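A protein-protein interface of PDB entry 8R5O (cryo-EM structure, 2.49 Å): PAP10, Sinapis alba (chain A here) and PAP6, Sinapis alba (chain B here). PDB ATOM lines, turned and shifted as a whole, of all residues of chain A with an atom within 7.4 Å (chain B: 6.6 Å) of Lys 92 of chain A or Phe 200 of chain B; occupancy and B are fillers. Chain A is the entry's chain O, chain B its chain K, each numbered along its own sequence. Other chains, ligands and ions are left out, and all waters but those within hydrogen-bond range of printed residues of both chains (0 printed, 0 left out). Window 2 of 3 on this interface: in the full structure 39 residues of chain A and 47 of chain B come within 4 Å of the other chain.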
ATOM      1  N   GLU A  86     -28.639 -13.775  -2.601  1.00  0.00           N
ATOM      2  CA  GLU A  86     -28.580 -12.521  -1.856  1.00  0.00           C
ATOM      3  C   GLU A  86     -29.370 -12.610  -0.557  1.00  0.00           C
ATOM      4  O   GLU A  86     -28.942 -12.079   0.474  1.00  0.00           O
ATOM      5  CB  GLU A  86     -29.091 -11.367  -2.719  1.00  0.00           C
ATOM      6  CG  GLU A  86     -28.161 -10.996  -3.864  1.00  0.00           C
ATOM      7  CD  GLU A  86     -28.699  -9.858  -4.714  1.00  0.00           C
ATOM      8  OE1 GLU A  86     -29.930  -9.655  -4.732  1.00  0.00           O
ATOM      9  OE2 GLU A  86     -27.885  -9.166  -5.362  1.00  0.00           O
ATOM     10  N   LEU A  87     -30.526 -13.276  -0.586  1.00  0.00           N
ATOM     11  CA  LEU A  87     -31.326 -13.418   0.627  1.00  0.00           C
ATOM     12  C   LEU A  87     -30.606 -14.265   1.669  1.00  0.00           C
ATOM     13  O   LEU A  87     -30.705 -13.994   2.869  1.00  0.00           O
ATOM     14  CB  LEU A  87     -32.689 -14.021   0.292  1.00  0.00           C
ATOM     15  CG  LEU A  87     -33.651 -14.184   1.469  1.00  0.00           C
ATOM     16  CD1 LEU A  87     -33.867 -12.855   2.171  1.00  0.00           C
ATOM     17  CD2 LEU A  87     -34.978 -14.769   1.013  1.00  0.00           C
ATOM     18  N   GLN A  88     -29.884 -15.298   1.229  1.00  0.00           N
ATOM     19  CA  GLN A  88     -29.171 -16.158   2.166  1.00  0.00           C
ATOM     20  C   GLN A  88     -28.096 -15.388   2.922  1.00  0.00           C
ATOM     21  O   GLN A  88     -27.954 -15.539   4.140  1.00  0.00           O
ATOM     22  CB  GLN A  88     -28.563 -17.349   1.426  1.00  0.00           C
ATOM     23  CG  GLN A  88     -27.861 -18.345   2.329  1.00  0.00           C
ATOM     24  CD  GLN A  88     -27.289 -19.521   1.568  1.00  0.00           C
ATOM     25  OE1 GLN A  88     -26.996 -19.422   0.377  1.00  0.00           O
ATOM     26  NE2 GLN A  88     -27.133 -20.647   2.252  1.00  0.00           N
ATOM     27  N   ASP A  89     -27.332 -14.551   2.217  1.00  0.00           N
ATOM     28  CA  ASP A  89     -26.320 -13.735   2.880  1.00  0.00           C
ATOM     29  C   ASP A  89     -26.959 -12.747   3.847  1.00  0.00           C
ATOM     30  O   ASP A  89     -26.415 -12.480   4.924  1.00  0.00           O
ATOM     31  CB  ASP A  89     -25.471 -13.002   1.844  1.00  0.00           C
ATOM     32  CG  ASP A  89     -24.701 -13.951   0.947  1.00  0.00           C
ATOM     33  OD1 ASP A  89     -24.475 -15.108   1.361  1.00  0.00           O
ATOM     34  OD2 ASP A  89     -24.320 -13.542  -0.170  1.00  0.00           O
ATOM     35  N   LEU A  90     -28.115 -12.192   3.478  1.00  0.00           N
ATOM     36  CA  LEU A  90     -28.812 -11.269   4.367  1.00  0.00           C
ATOM     37  C   LEU A  90     -29.283 -11.972   5.633  1.00  0.00           C
ATOM     38  O   LEU A  90     -29.290 -11.374   6.717  1.00  0.00           O
ATOM     39  CB  LEU A  90     -29.990 -10.630   3.632  1.00  0.00           C
ATOM     40  CG  LEU A  90     -30.718  -9.495   4.351  1.00  0.00           C
ATOM     41  CD1 LEU A  90     -29.763  -8.346   4.630  1.00  0.00           C
ATOM     42  CD2 LEU A  90     -31.907  -9.021   3.535  1.00  0.00           C
ATOM     43  N   VAL A  91     -29.678 -13.241   5.522  1.00  0.00           N
ATOM     44  CA  VAL A  91     -30.130 -13.981   6.699  1.00  0.00           C
ATOM     45  C   VAL A  91     -28.941 -14.436   7.537  1.00  0.00           C
ATOM     46  O   VAL A  91     -28.966 -14.351   8.770  1.00  0.00           O
ATOM     47  CB  VAL A  91     -31.020 -15.165   6.280  1.00  0.00           C
ATOM     48  CG1 VAL A  91     -31.376 -16.016   7.485  1.00  0.00           C
ATOM     49  CG2 VAL A  91     -32.280 -14.662   5.597  1.00  0.00           C
ATOM     50  N   LYS A  92     -27.881 -14.926   6.886  1.00  0.00           N
ATOM     51  CA  LYS A  92     -26.691 -15.343   7.622  1.00  0.00           C
ATOM     52  C   LYS A  92     -26.018 -14.163   8.311  1.00  0.00           C
ATOM     53  O   LYS A  92     -25.525 -14.294   9.435  1.00  0.00           O
ATOM     54  CB  LYS A  92     -25.708 -16.045   6.686  1.00  0.00           C
ATOM     55  CG  LYS A  92     -25.822 -17.557   6.692  1.00  0.00           C
ATOM     56  CD  LYS A  92     -24.686 -18.198   5.920  1.00  0.00           C
ATOM     57  CE  LYS A  92     -24.730 -19.711   6.033  1.00  0.00           C
ATOM     58  NZ  LYS A  92     -23.617 -20.357   5.284  1.00  0.00           N
ATOM     59  N   GLY A  93     -25.987 -13.008   7.655  1.00  0.00           N
ATOM     60  CA  GLY A  93     -25.352 -11.839   8.227  1.00  0.00           C
ATOM     61  C   GLY A  93     -26.069 -11.342   9.467  1.00  0.00           C
ATOM     62  O   GLY A  93     -27.137 -11.816   9.856  1.00  0.00           O
ATOM     63  N   GLU A  94     -25.452 -10.351  10.105  1.00  0.00           N
ATOM     64  CA  GLU A  94     -25.989  -9.790  11.336  1.00  0.00           C
ATOM     65  C   GLU A  94     -27.072  -8.769  11.014  1.00  0.00           C
ATOM     66  O   GLU A  94     -26.875  -7.885  10.174  1.00  0.00           O
ATOM     67  CB  GLU A  94     -24.877  -9.142  12.158  1.00  0.00           C
ATOM     68  CG  GLU A  94     -25.300  -8.735  13.562  1.00  0.00           C
ATOM     69  CD  GLU A  94     -25.565  -9.929  14.459  1.00  0.00           C
ATOM     70  OE1 GLU A  94     -25.017 -11.017  14.183  1.00  0.00           O
ATOM     71  OE2 GLU A  94     -26.323  -9.781  15.440  1.00  0.00           O
ATOM     72  N   ARG A  95     -28.212  -8.892  11.684  1.00  0.00           N
ATOM     73  CA  ARG A  95     -29.345  -8.008  11.469  1.00  0.00           C
ATOM     74  C   ARG A  95     -29.800  -7.422  12.795  1.00  0.00           C
ATOM     75  O   ARG A  95     -29.684  -8.056  13.847  1.00  0.00           O
ATOM     76  CB  ARG A  95     -30.512  -8.745  10.799  1.00  0.00           C
ATOM     77  CG  ARG A  95     -30.258  -9.133   9.355  1.00  0.00           C
ATOM     78  CD  ARG A  95     -31.295 -10.126   8.857  1.00  0.00           C
ATOM     79  NE  ARG A  95     -31.118 -11.445   9.452  1.00  0.00           N
ATOM     80  CZ  ARG A  95     -31.828 -11.909  10.470  1.00  0.00           C
ATOM     81  NH1 ARG A  95     -32.789 -11.192  11.029  1.00  0.00           N
ATOM     82  NH2 ARG A  95     -31.569 -13.127  10.938  1.00  0.00           N
ATOM     83  N   LEU A  99     -36.872  -8.734   9.592  1.00  0.00           N
ATOM     84  CA  LEU A  99     -36.757  -8.994   8.163  1.00  0.00           C
ATOM     85  C   LEU A  99     -38.038  -9.659   7.676  1.00  0.00           C
ATOM     86  O   LEU A  99     -38.405 -10.736   8.158  1.00  0.00           O
ATOM     87  CB  LEU A  99     -35.545  -9.876   7.868  1.00  0.00           C
ATOM     88  CG  LEU A  99     -35.315 -10.273   6.411  1.00  0.00           C
ATOM     89  CD1 LEU A  99     -35.133  -9.040   5.544  1.00  0.00           C
ATOM     90  CD2 LEU A  99     -34.116 -11.200   6.289  1.00  0.00           C
ATOM     91  N   ILE B 198     -35.280 -21.839  10.300  1.00  0.00           N
ATOM     92  CA  ILE B 198     -34.483 -21.693   9.088  1.00  0.00           C
ATOM     93  C   ILE B 198     -33.149 -22.400   9.285  1.00  0.00           C
ATOM     94  O   ILE B 198     -32.446 -22.155  10.273  1.00  0.00           O
ATOM     95  CB  ILE B 198     -34.282 -20.209   8.740  1.00  0.00           C
ATOM     96  CG1 ILE B 198     -35.640 -19.525   8.575  1.00  0.00           C
ATOM     97  CG2 ILE B 198     -33.454 -20.066   7.477  1.00  0.00           C
ATOM     98  CD1 ILE B 198     -35.556 -18.062   8.240  1.00  0.00           C
ATOM     99  N   LYS B 199     -32.808 -23.283   8.353  1.00  0.00           N
ATOM    100  CA  LYS B 199     -31.546 -24.008   8.361  1.00  0.00           C
ATOM    101  C   LYS B 199     -30.777 -23.709   7.080  1.00  0.00           C
ATOM    102  O   LYS B 199     -31.319 -23.172   6.111  1.00  0.00           O
ATOM    103  CB  LYS B 199     -31.770 -25.520   8.511  1.00  0.00           C
ATOM    104  CG  LYS B 199     -32.610 -26.146   7.410  1.00  0.00           C
ATOM    105  CD  LYS B 199     -32.555 -27.668   7.472  1.00  0.00           C
ATOM    106  CE  LYS B 199     -32.954 -28.187   8.846  1.00  0.00           C
ATOM    107  NZ  LYS B 199     -32.922 -29.675   8.918  1.00  0.00           N
ATOM    108  N   PHE B 200     -29.495 -24.066   7.085  1.00  0.00           N
ATOM    109  CA  PHE B 200     -28.576 -23.781   5.986  1.00  0.00           C
ATOM    110  C   PHE B 200     -27.902 -25.059   5.509  1.00  0.00           C
ATOM    111  O   PHE B 200     -26.679 -25.146   5.388  1.00  0.00           O
ATOM    112  CB  PHE B 200     -27.546 -22.735   6.396  1.00  0.00           C
ATOM    113  CG  PHE B 200     -28.119 -21.361   6.559  1.00  0.00           C
ATOM    114  CD1 PHE B 200     -28.324 -20.549   5.457  1.00  0.00           C
ATOM    115  CD2 PHE B 200     -28.463 -20.882   7.810  1.00  0.00           C
ATOM    116  CE1 PHE B 200     -28.855 -19.285   5.602  1.00  0.00           C
ATOM    117  CE2 PHE B 200     -28.994 -19.620   7.960  1.00  0.00           C
ATOM    118  CZ  PHE B 200     -29.191 -18.820   6.856  1.00  0.00           C
ATOM    119  N   GLU B 201     -28.711 -26.080   5.239  1.00  0.00           N
ATOM    120  CA  GLU B 201     -28.184 -27.370   4.816  1.00  0.00           C
ATOM    121  C   GLU B 201     -27.534 -27.275   3.441  1.00  0.00           C
ATOM    122  O   GLU B 201     -28.059 -26.624   2.532  1.00  0.00           O
ATOM    123  CB  GLU B 201     -29.304 -28.411   4.796  1.00  0.00           C
ATOM    124  CG  GLU B 201     -28.820 -29.849   4.763  1.00  0.00           C
ATOM    125  CD  GLU B 201     -29.962 -30.845   4.801  1.00  0.00           C
ATOM    126  OE1 GLU B 201     -31.115 -30.441   4.542  1.00  0.00           O
ATOM    127  OE2 GLU B 201     -29.705 -32.031   5.094  1.00  0.00           O
ATOM    128  N   ASP B 202     -26.392 -27.949   3.300  1.00  0.00           N
ATOM    129  CA  ASP B 202     -25.610 -28.039   2.059  1.00  0.00           C
ATOM    130  C   ASP B 202     -25.572 -26.712   1.301  1.00  0.00           C
ATOM    131  O   ASP B 202     -25.828 -26.640   0.097  1.00  0.00           O
ATOM    132  CB  ASP B 202     -26.114 -29.176   1.161  1.00  0.00           C
ATOM    133  CG  ASP B 202     -27.575 -29.028   0.767  1.00  0.00           C
ATOM    134  OD1 ASP B 202     -28.456 -29.321   1.601  1.00  0.00           O
ATOM    135  OD2 ASP B 202     -27.841 -28.623  -0.383  1.00  0.00           O
ATOM    136  N   GLY B 203     -25.235 -25.647   2.026  1.00  0.00           N
ATOM    137  CA  GLY B 203     -25.061 -24.348   1.407  1.00  0.00           C
ATOM    138  C   GLY B 203     -26.315 -23.722   0.847  1.00  0.00           C
ATOM    139  O   GLY B 203     -26.223 -22.791   0.043  1.00  0.00           O
ATOM    140  N   LYS B 204     -27.490 -24.203   1.244  1.00  0.00           N
ATOM    141  CA  LYS B 204     -28.756 -23.665   0.770  1.00  0.00           C
ATOM    142  C   LYS B 204     -29.683 -23.431   1.953  1.00  0.00           C
ATOM    143  O   LYS B 204     -29.604 -24.125   2.969  1.00  0.00           O
ATOM    144  CB  LYS B 204     -29.429 -24.602  -0.242  1.00  0.00           C
ATOM    145  CG  LYS B 204     -28.628 -24.828  -1.514  1.00  0.00           C
ATOM    146  CD  LYS B 204     -29.460 -25.547  -2.566  1.00  0.00           C
ATOM    147  CE  LYS B 204     -30.029 -26.847  -2.026  1.00  0.00           C
ATOM    148  NZ  LYS B 204     -30.879 -27.543  -3.033  1.00  0.00           N
ATOM    149  N   MET B 205     -30.567 -22.448   1.810  1.00  0.00           N
ATOM    150  CA  MET B 205     -31.474 -22.065   2.880  1.00  0.00           C
ATOM    151  C   MET B 205     -32.755 -22.884   2.795  1.00  0.00           C
ATOM    152  O   MET B 205     -33.412 -22.915   1.750  1.00  0.00           O
ATOM    153  CB  MET B 205     -31.797 -20.572   2.806  1.00  0.00           C
ATOM    154  CG  MET B 205     -32.009 -19.923   4.161  1.00  0.00           C
ATOM    155  SD  MET B 205     -33.082 -18.476   4.125  1.00  0.00           S
ATOM    156  CE  MET B 205     -32.467 -17.630   2.677  1.00  0.00           C
ATOM    157  N   LYS B 206     -33.103 -23.547   3.894  1.00  0.00           N
ATOM    158  CA  LYS B 206     -34.323 -24.333   3.983  1.00  0.00           C
ATOM    159  C   LYS B 206     -35.048 -23.994   5.276  1.00  0.00           C
ATOM    160  O   LYS B 206     -34.476 -23.412   6.201  1.00  0.00           O
ATOM    161  CB  LYS B 206     -34.038 -25.840   3.927  1.00  0.00           C
ATOM    162  CG  LYS B 206     -33.283 -26.293   2.691  1.00  0.00           C
ATOM    163  CD  LYS B 206     -33.077 -27.798   2.695  1.00  0.00           C
ATOM    164  CE  LYS B 206     -32.153 -28.235   1.571  1.00  0.00           C
ATOM    165  NZ  LYS B 206     -32.664 -27.817   0.237  1.00  0.00           N
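The backbone carbonyl oxygen (O) of Gly 203 of chain B is in hydrogen-bond range of the side-chain amide nitrogen (NE2) of Gln 88 of chain A (3.2 Å).
Met 205 of chain B touches Leu 87 of chain A (CE to CG, 3.8 Å).
Gln 88 of chain A touches Phe 200 of chain B (NE2 to CD1, 3.4 Å).
Gln 88 of chain A touches Lys 204 of chain B.
CA of Gln 88 of chain A touches CE of Met 205 of chain B (3.6 Å).
CG1 of Val 91 of chain A touches CZ of Phe 200 of chain B (3.6 Å).
Lys 92 of chain A touches Phe 200 of chain B.
Phe 200 of chain B touches just these residues of chain A: Gln 88, Val 91 and Lys 92.
Printed residues of chain A within 4 Å of Gly 203 of chain B: Gln 88 (3.2 Å).
Of the printed residues of chain A, Lys 204 of chain B touches Gln 88.
Leu 90 of chain A touches none of the printed residues of chain B.
Lys 206 of chain B touches none of the printed residues of chain A.
The nearest residue of chain B that does not touch Lys 92 of chain A is Gly 203 of chain B (5.7 Å).
Of the 11 printed residues of chain A, 4 touch a printed residue of chain B.
Hydrophobic or aromatic side chains of chain A within 4 Å of the printed part of chain B: Leu 87 and Val 91.
Along chain B the printed residues that touch a printed residue of chain A span positions 200 to 205.
Among the printed residues, 7 pairs touch across the chains.
Among the printed residues, no Asp or Glu carboxylate lies within 4 Å of a Lys or Arg side-chain nitrogen of the other chain.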
